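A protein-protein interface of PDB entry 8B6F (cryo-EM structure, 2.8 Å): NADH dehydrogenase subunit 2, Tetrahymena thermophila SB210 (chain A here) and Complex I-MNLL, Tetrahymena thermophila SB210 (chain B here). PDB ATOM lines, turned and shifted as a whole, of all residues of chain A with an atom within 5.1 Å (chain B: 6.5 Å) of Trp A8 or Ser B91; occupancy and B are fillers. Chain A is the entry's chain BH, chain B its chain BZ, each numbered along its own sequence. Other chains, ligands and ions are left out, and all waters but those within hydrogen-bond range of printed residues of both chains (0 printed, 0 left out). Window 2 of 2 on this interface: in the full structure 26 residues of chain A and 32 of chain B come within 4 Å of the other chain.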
ATOM      1  N   MET A   1     -30.381 -30.130 -20.753  1.00  0.00           N
ATOM      2  CA  MET A   1     -29.458 -29.120 -21.342  1.00  0.00           C
ATOM      3  C   MET A   1     -28.125 -29.756 -21.706  1.00  0.00           C
ATOM      4  O   MET A   1     -27.359 -30.149 -20.829  1.00  0.00           O
ATOM      5  CB  MET A   1     -29.226 -27.963 -20.367  1.00  0.00           C
ATOM      6  CG  MET A   1     -30.495 -27.238 -19.941  1.00  0.00           C
ATOM      7  SD  MET A   1     -31.428 -26.538 -21.317  1.00  0.00           S
ATOM      8  CE  MET A   1     -30.214 -25.451 -22.058  1.00  0.00           C
ATOM      9  N   SER A   2     -27.852 -29.853 -23.005  1.00  0.00           N
ATOM     10  CA  SER A   2     -26.607 -30.411 -23.507  1.00  0.00           C
ATOM     11  C   SER A   2     -26.016 -29.471 -24.546  1.00  0.00           C
ATOM     12  O   SER A   2     -26.744 -28.804 -25.284  1.00  0.00           O
ATOM     13  CB  SER A   2     -26.819 -31.797 -24.124  1.00  0.00           C
ATOM     14  OG  SER A   2     -27.394 -32.692 -23.188  1.00  0.00           O
ATOM     15  N   ILE A   3     -24.688 -29.427 -24.598  1.00  0.00           N
ATOM     16  CA  ILE A   3     -23.959 -28.552 -25.508  1.00  0.00           C
ATOM     17  C   ILE A   3     -23.156 -29.425 -26.460  1.00  0.00           C
ATOM     18  O   ILE A   3     -22.369 -30.272 -26.020  1.00  0.00           O
ATOM     19  CB  ILE A   3     -23.025 -27.590 -24.751  1.00  0.00           C
ATOM     20  CG1 ILE A   3     -23.739 -26.992 -23.538  1.00  0.00           C
ATOM     21  CG2 ILE A   3     -22.559 -26.485 -25.688  1.00  0.00           C
ATOM     22  CD1 ILE A   3     -22.864 -26.079 -22.700  1.00  0.00           C
ATOM     23  N   ASN A   6     -21.509 -25.690 -29.284  1.00  0.00           N
ATOM     24  CA  ASN A   6     -22.254 -24.467 -29.018  1.00  0.00           C
ATOM     25  C   ASN A   6     -23.709 -24.553 -29.460  1.00  0.00           C
ATOM     26  O   ASN A   6     -24.366 -23.522 -29.625  1.00  0.00           O
ATOM     27  CB  ASN A   6     -21.584 -23.262 -29.687  1.00  0.00           C
ATOM     28  CG  ASN A   6     -20.107 -23.171 -29.368  1.00  0.00           C
ATOM     29  OD1 ASN A   6     -19.713 -22.582 -28.363  1.00  0.00           O
ATOM     30  ND2 ASN A   6     -19.279 -23.758 -30.226  1.00  0.00           N
ATOM     31  N   ILE A   7     -24.231 -25.759 -29.660  1.00  0.00           N
ATOM     32  CA  ILE A   7     -25.643 -25.977 -29.958  1.00  0.00           C
ATOM     33  C   ILE A   7     -26.289 -26.562 -28.712  1.00  0.00           C
ATOM     34  O   ILE A   7     -25.946 -27.673 -28.290  1.00  0.00           O
ATOM     35  CB  ILE A   7     -25.840 -26.899 -31.174  1.00  0.00           C
ATOM     36  CG1 ILE A   7     -25.765 -26.104 -32.480  1.00  0.00           C
ATOM     37  CG2 ILE A   7     -27.181 -27.627 -31.112  1.00  0.00           C
ATOM     38  CD1 ILE A   7     -24.418 -25.489 -32.756  1.00  0.00           C
ATOM     39  N   TRP A   8     -27.213 -25.814 -28.118  1.00  0.00           N
ATOM     40  CA  TRP A   8     -27.904 -26.276 -26.925  1.00  0.00           C
ATOM     41  C   TRP A   8     -29.048 -27.208 -27.297  1.00  0.00           C
ATOM     42  O   TRP A   8     -29.779 -26.966 -28.260  1.00  0.00           O
ATOM     43  CB  TRP A   8     -28.453 -25.094 -26.133  1.00  0.00           C
ATOM     44  CG  TRP A   8     -27.395 -24.219 -25.590  1.00  0.00           C
ATOM     45  CD1 TRP A   8     -26.812 -23.171 -26.225  1.00  0.00           C
ATOM     46  CD2 TRP A   8     -26.784 -24.303 -24.299  1.00  0.00           C
ATOM     47  NE1 TRP A   8     -25.876 -22.593 -25.414  1.00  0.00           N
ATOM     48  CE2 TRP A   8     -25.835 -23.269 -24.223  1.00  0.00           C
ATOM     49  CE3 TRP A   8     -26.945 -25.154 -23.201  1.00  0.00           C
ATOM     50  CZ2 TRP A   8     -25.050 -23.059 -23.093  1.00  0.00           C
ATOM     51  CZ3 TRP A   8     -26.164 -24.945 -22.079  1.00  0.00           C
ATOM     52  CH2 TRP A   8     -25.228 -23.904 -22.033  1.00  0.00           C
ATOM     53  N   ILE A   9     -29.194 -28.281 -26.527  1.00  0.00           N
ATOM     54  CA  ILE A   9     -30.270 -29.244 -26.709  1.00  0.00           C
ATOM     55  C   ILE A   9     -30.984 -29.397 -25.376  1.00  0.00           C
ATOM     56  O   ILE A   9     -30.348 -29.685 -24.357  1.00  0.00           O
ATOM     57  CB  ILE A   9     -29.751 -30.603 -27.211  1.00  0.00           C
ATOM     58  CG1 ILE A   9     -28.960 -30.405 -28.507  1.00  0.00           C
ATOM     59  CG2 ILE A   9     -30.910 -31.569 -27.415  1.00  0.00           C
ATOM     60  CD1 ILE A   9     -28.348 -31.667 -29.054  1.00  0.00           C
ATOM     61  N   ASN A  10     -32.299 -29.208 -25.385  1.00  0.00           N
ATOM     62  CA  ASN A  10     -33.114 -29.253 -24.176  1.00  0.00           C
ATOM     63  C   ASN A  10     -34.206 -30.297 -24.364  1.00  0.00           C
ATOM     64  O   ASN A  10     -35.146 -30.090 -25.137  1.00  0.00           O
ATOM     65  CB  ASN A  10     -33.707 -27.879 -23.865  1.00  0.00           C
ATOM     66  CG  ASN A  10     -34.160 -27.144 -25.107  1.00  0.00           C
ATOM     67  OD1 ASN A  10     -34.507 -27.758 -26.115  1.00  0.00           O
ATOM     68  ND2 ASN A  10     -34.149 -25.818 -25.045  1.00  0.00           N
ATOM     69  N   GLN B  70     -34.941 -21.130 -22.175  1.00  0.00           N
ATOM     70  CA  GLN B  70     -34.098 -22.091 -21.472  1.00  0.00           C
ATOM     71  C   GLN B  70     -32.623 -21.856 -21.769  1.00  0.00           C
ATOM     72  O   GLN B  70     -31.786 -21.907 -20.862  1.00  0.00           O
ATOM     73  CB  GLN B  70     -34.497 -23.516 -21.857  1.00  0.00           C
ATOM     74  CG  GLN B  70     -35.782 -24.002 -21.210  1.00  0.00           C
ATOM     75  CD  GLN B  70     -35.625 -24.252 -19.725  1.00  0.00           C
ATOM     76  OE1 GLN B  70     -35.471 -23.318 -18.940  1.00  0.00           O
ATOM     77  NE2 GLN B  70     -35.655 -25.519 -19.333  1.00  0.00           N
ATOM     78  N   ILE B  71     -32.285 -21.607 -23.034  1.00  0.00           N
ATOM     79  CA  ILE B  71     -30.886 -21.396 -23.400  1.00  0.00           C
ATOM     80  C   ILE B  71     -30.337 -20.155 -22.707  1.00  0.00           C
ATOM     81  O   ILE B  71     -29.239 -20.172 -22.141  1.00  0.00           O
ATOM     82  CB  ILE B  71     -30.741 -21.302 -24.930  1.00  0.00           C
ATOM     83  CG1 ILE B  71     -31.147 -22.627 -25.579  1.00  0.00           C
ATOM     84  CG2 ILE B  71     -29.311 -20.939 -25.311  1.00  0.00           C
ATOM     85  CD1 ILE B  71     -31.242 -22.575 -27.090  1.00  0.00           C
ATOM     86  N   LYS B  74     -30.206 -20.633 -18.879  1.00  0.00           N
ATOM     87  CA  LYS B  74     -29.059 -21.441 -18.477  1.00  0.00           C
ATOM     88  C   LYS B  74     -27.792 -20.601 -18.398  1.00  0.00           C
ATOM     89  O   LYS B  74     -27.012 -20.730 -17.448  1.00  0.00           O
ATOM     90  CB  LYS B  74     -28.875 -22.597 -19.461  1.00  0.00           C
ATOM     91  CG  LYS B  74     -27.733 -23.545 -19.129  1.00  0.00           C
ATOM     92  CD  LYS B  74     -28.009 -24.331 -17.861  1.00  0.00           C
ATOM     93  CE  LYS B  74     -26.934 -25.379 -17.621  1.00  0.00           C
ATOM     94  NZ  LYS B  74     -27.237 -26.223 -16.434  1.00  0.00           N
ATOM     95  N   LEU B  75     -27.570 -19.736 -19.388  1.00  0.00           N
ATOM     96  CA  LEU B  75     -26.366 -18.910 -19.390  1.00  0.00           C
ATOM     97  C   LEU B  75     -26.357 -17.941 -18.216  1.00  0.00           C
ATOM     98  O   LEU B  75     -25.310 -17.705 -17.605  1.00  0.00           O
ATOM     99  CB  LEU B  75     -26.252 -18.153 -20.713  1.00  0.00           C
ATOM    100  CG  LEU B  75     -26.058 -19.008 -21.967  1.00  0.00           C
ATOM    101  CD1 LEU B  75     -26.044 -18.137 -23.208  1.00  0.00           C
ATOM    102  CD2 LEU B  75     -24.781 -19.823 -21.886  1.00  0.00           C
ATOM    103  N   LEU B  78     -25.422 -19.509 -14.770  1.00  0.00           N
ATOM    104  CA  LEU B  78     -24.049 -19.931 -14.536  1.00  0.00           C
ATOM    105  C   LEU B  78     -23.488 -19.264 -13.290  1.00  0.00           C
ATOM    106  O   LEU B  78     -23.687 -18.068 -13.060  1.00  0.00           O
ATOM    107  CB  LEU B  78     -23.179 -19.591 -15.747  1.00  0.00           C
ATOM    108  CG  LEU B  78     -23.580 -20.246 -17.069  1.00  0.00           C
ATOM    109  CD1 LEU B  78     -22.736 -19.700 -18.205  1.00  0.00           C
ATOM    110  CD2 LEU B  78     -23.450 -21.755 -16.985  1.00  0.00           C
ATOM    111  N   ALA B  87     -15.879 -24.049 -21.148  1.00  0.00           N
ATOM    112  CA  ALA B  87     -17.094 -24.791 -21.458  1.00  0.00           C
ATOM    113  C   ALA B  87     -18.278 -23.897 -21.789  1.00  0.00           C
ATOM    114  O   ALA B  87     -19.267 -24.389 -22.345  1.00  0.00           O
ATOM    115  CB  ALA B  87     -17.470 -25.699 -20.284  1.00  0.00           C
ATOM    116  N   TYR B  88     -18.211 -22.605 -21.464  1.00  0.00           N
ATOM    117  CA  TYR B  88     -19.315 -21.689 -21.712  1.00  0.00           C
ATOM    118  C   TYR B  88     -18.889 -20.374 -22.345  1.00  0.00           C
ATOM    119  O   TYR B  88     -19.763 -19.573 -22.694  1.00  0.00           O
ATOM    120  CB  TYR B  88     -20.057 -21.379 -20.403  1.00  0.00           C
ATOM    121  CG  TYR B  88     -20.654 -22.591 -19.728  1.00  0.00           C
ATOM    122  CD1 TYR B  88     -21.782 -23.213 -20.244  1.00  0.00           C
ATOM    123  CD2 TYR B  88     -20.099 -23.103 -18.563  1.00  0.00           C
ATOM    124  CE1 TYR B  88     -22.334 -24.317 -19.627  1.00  0.00           C
ATOM    125  CE2 TYR B  88     -20.643 -24.207 -17.937  1.00  0.00           C
ATOM    126  CZ  TYR B  88     -21.761 -24.809 -18.475  1.00  0.00           C
ATOM    127  OH  TYR B  88     -22.310 -25.907 -17.858  1.00  0.00           O
ATOM    128  N   ARG B  89     -17.589 -20.126 -22.513  1.00  0.00           N
ATOM    129  CA  ARG B  89     -17.134 -18.824 -22.994  1.00  0.00           C
ATOM    130  C   ARG B  89     -17.651 -18.541 -24.399  1.00  0.00           C
ATOM    131  O   ARG B  89     -18.150 -17.446 -24.681  1.00  0.00           O
ATOM    132  CB  ARG B  89     -15.608 -18.762 -22.957  1.00  0.00           C
ATOM    133  CG  ARG B  89     -15.027 -17.518 -23.599  1.00  0.00           C
ATOM    134  CD  ARG B  89     -13.552 -17.367 -23.274  1.00  0.00           C
ATOM    135  NE  ARG B  89     -12.832 -18.623 -23.447  1.00  0.00           N
ATOM    136  CZ  ARG B  89     -12.361 -19.070 -24.603  1.00  0.00           C
ATOM    137  NH1 ARG B  89     -12.522 -18.389 -25.725  1.00  0.00           N
ATOM    138  NH2 ARG B  89     -11.718 -20.233 -24.634  1.00  0.00           N
ATOM    139  N   GLU B  90     -17.537 -19.518 -25.297  1.00  0.00           N
ATOM    140  CA  GLU B  90     -17.953 -19.299 -26.678  1.00  0.00           C
ATOM    141  C   GLU B  90     -19.453 -19.064 -26.766  1.00  0.00           C
ATOM    142  O   GLU B  90     -19.908 -18.177 -27.497  1.00  0.00           O
ATOM    143  CB  GLU B  90     -17.544 -20.487 -27.545  1.00  0.00           C
ATOM    144  CG  GLU B  90     -17.850 -20.296 -29.019  1.00  0.00           C
ATOM    145  CD  GLU B  90     -17.344 -21.442 -29.867  1.00  0.00           C
ATOM    146  OE1 GLU B  90     -16.632 -22.313 -29.324  1.00  0.00           O
ATOM    147  OE2 GLU B  90     -17.661 -21.476 -31.074  1.00  0.00           O
ATOM    148  N   SER B  91     -20.238 -19.855 -26.036  1.00  0.00           N
ATOM    149  CA  SER B  91     -21.684 -19.676 -26.046  1.00  0.00           C
ATOM    150  C   SER B  91     -22.085 -18.338 -25.440  1.00  0.00           C
ATOM    151  O   SER B  91     -22.991 -17.668 -25.946  1.00  0.00           O
ATOM    152  CB  SER B  91     -22.339 -20.813 -25.271  1.00  0.00           C
ATOM    153  OG  SER B  91     -23.743 -20.700 -25.291  1.00  0.00           O
ATOM    154  N   PHE B  92     -21.425 -17.934 -24.356  1.00  0.00           N
ATOM    155  CA  PHE B  92     -21.729 -16.645 -23.747  1.00  0.00           C
ATOM    156  C   PHE B  92     -21.442 -15.500 -24.708  1.00  0.00           C
ATOM    157  O   PHE B  92     -22.235 -14.559 -24.821  1.00  0.00           O
ATOM    158  CB  PHE B  92     -20.934 -16.478 -22.454  1.00  0.00           C
ATOM    159  CG  PHE B  92     -21.193 -15.180 -21.753  1.00  0.00           C
ATOM    160  CD1 PHE B  92     -22.227 -15.063 -20.843  1.00  0.00           C
ATOM    161  CD2 PHE B  92     -20.395 -14.075 -22.003  1.00  0.00           C
ATOM    162  CE1 PHE B  92     -22.468 -13.867 -20.197  1.00  0.00           C
ATOM    163  CE2 PHE B  92     -20.629 -12.876 -21.361  1.00  0.00           C
ATOM    164  CZ  PHE B  92     -21.667 -12.772 -20.455  1.00  0.00           C
ATOM    165  N   PHE B  93     -20.314 -15.565 -25.416  1.00  0.00           N
ATOM    166  CA  PHE B  93     -20.004 -14.537 -26.402  1.00  0.00           C
ATOM    167  C   PHE B  93     -20.989 -14.567 -27.563  1.00  0.00           C
ATOM    168  O   PHE B  93     -21.328 -13.517 -28.119  1.00  0.00           O
ATOM    169  CB  PHE B  93     -18.572 -14.709 -26.911  1.00  0.00           C
ATOM    170  CG  PHE B  93     -17.516 -14.297 -25.921  1.00  0.00           C
ATOM    171  CD1 PHE B  93     -17.722 -13.233 -25.054  1.00  0.00           C
ATOM    172  CD2 PHE B  93     -16.309 -14.972 -25.865  1.00  0.00           C
ATOM    173  CE1 PHE B  93     -16.749 -12.859 -24.151  1.00  0.00           C
ATOM    174  CE2 PHE B  93     -15.333 -14.600 -24.963  1.00  0.00           C
ATOM    175  CZ  PHE B  93     -15.554 -13.542 -24.106  1.00  0.00           C
ATOM    176  N   GLU B  94     -21.454 -15.755 -27.952  1.00  0.00           N
ATOM    177  CA  GLU B  94     -22.455 -15.825 -29.010  1.00  0.00           C
ATOM    178  C   GLU B  94     -23.739 -15.118 -28.599  1.00  0.00           C
ATOM    179  O   GLU B  94     -24.340 -14.392 -29.399  1.00  0.00           O
ATOM    180  CB  GLU B  94     -22.737 -17.286 -29.365  1.00  0.00           C
ATOM    181  CG  GLU B  94     -23.839 -17.467 -30.399  1.00  0.00           C
ATOM    182  CD  GLU B  94     -24.066 -18.921 -30.761  1.00  0.00           C
ATOM    183  OE1 GLU B  94     -23.215 -19.764 -30.410  1.00  0.00           O
ATOM    184  OE2 GLU B  94     -25.099 -19.221 -31.395  1.00  0.00           O
ATOM    185  N   HIS B  95     -24.182 -15.319 -27.359  1.00  0.00           N
ATOM    186  CA  HIS B  95     -25.424 -14.708 -26.903  1.00  0.00           C
ATOM    187  C   HIS B  95     -25.257 -13.254 -26.486  1.00  0.00           C
ATOM    188  O   HIS B  95     -26.259 -12.542 -26.370  1.00  0.00           O
ATOM    189  CB  HIS B  95     -26.006 -15.508 -25.738  1.00  0.00           C
ATOM    190  CG  HIS B  95     -26.790 -16.707 -26.168  1.00  0.00           C
ATOM    191  ND1 HIS B  95     -26.194 -17.900 -26.517  1.00  0.00           N
ATOM    192  CD2 HIS B  95     -28.122 -16.895 -26.316  1.00  0.00           C
ATOM    193  CE1 HIS B  95     -27.127 -18.772 -26.857  1.00  0.00           C
ATOM    194  NE2 HIS B  95     -28.305 -18.187 -26.745  1.00  0.00           N
ATOM    195  N   ALA B  96     -24.027 -12.796 -26.257  1.00  0.00           N
ATOM    196  CA  ALA B  96     -23.789 -11.427 -25.824  1.00  0.00           C
ATOM    197  C   ALA B  96     -23.296 -10.516 -26.939  1.00  0.00           C
ATOM    198  O   ALA B  96     -23.318  -9.293 -26.766  1.00  0.00           O
ATOM    199  CB  ALA B  96     -22.773 -11.405 -24.677  1.00  0.00           C
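Ser A2 touches none of the printed residues of chain B.
Of the printed residues of chain B, Trp A8 touches Ile B71 (3.5 Å), Lys B74 (3.6 Å), Leu B75 (3.5 Å), Tyr B88 (3.8 Å) and Ser B91 (2.9 Å).
Printed residues of chain A within 4 Å of Tyr B88: Ile A3 and Trp A8.
Ser B91 touches two residues of chain A.
Of the printed residues of chain A, Glu B94 touches Asn A6 (3.9 Å).
The nearest residue of chain B that does not touch Trp A8 is His B95 (4.3 Å).
The nearest printed residue of chain A that does not touch Ala B87 is Trp A8 (6.0 Å).
Of the 8 printed residues of chain A, 4 touch a printed residue of chain B.
Along chain A the printed residues that touch a printed residue of chain B span positions 3 to 10.
Along chain B the printed residues that touch a printed residue of chain A span positions 70 to 94.
Among the printed residues, 11 pairs touch across the chains.
Among the printed residues, no Asp or Glu carboxylate lies within 4 Å of a Lys or Arg side-chain nitrogen of the other chain.
Ala B87 touches Ile A3 (O to CD1, 3.99 Å).
CD1 of Ile A3 touches CE1 of Tyr B88 (3.6 Å).
Ser B91 touches Asn A6 (N to OD1, 3.6 Å).
OE1 of Glu B94 touches CB of Asn A6, 3.9 Å away.
CG2 of Ile B71 touches CD1 of Trp A8, at 3.5 Å.
CZ3 of Trp A8 touches CG of Lys B74 (3.6 Å).
Trp A8 touches Leu B75 (CZ2 to CD2, 3.5 Å).
Tyr B88 touches Trp A8 (CE1 to CH2, 3.8 Å).
Gln B70 touches Asn A10.
ND1 of His B95 is in hydrogen-bond range of O of Ser B91 (3.3 Å).
OE2 of Glu B90 sits at hydrogen-bond distance from ND2 of Asn A6 (2.9 Å).
The indole nitrogen (NE1) of Trp A8 lies within hydrogen-bond range of the side-chain hydroxyl (OG) of Ser B91 (2.9 Å).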
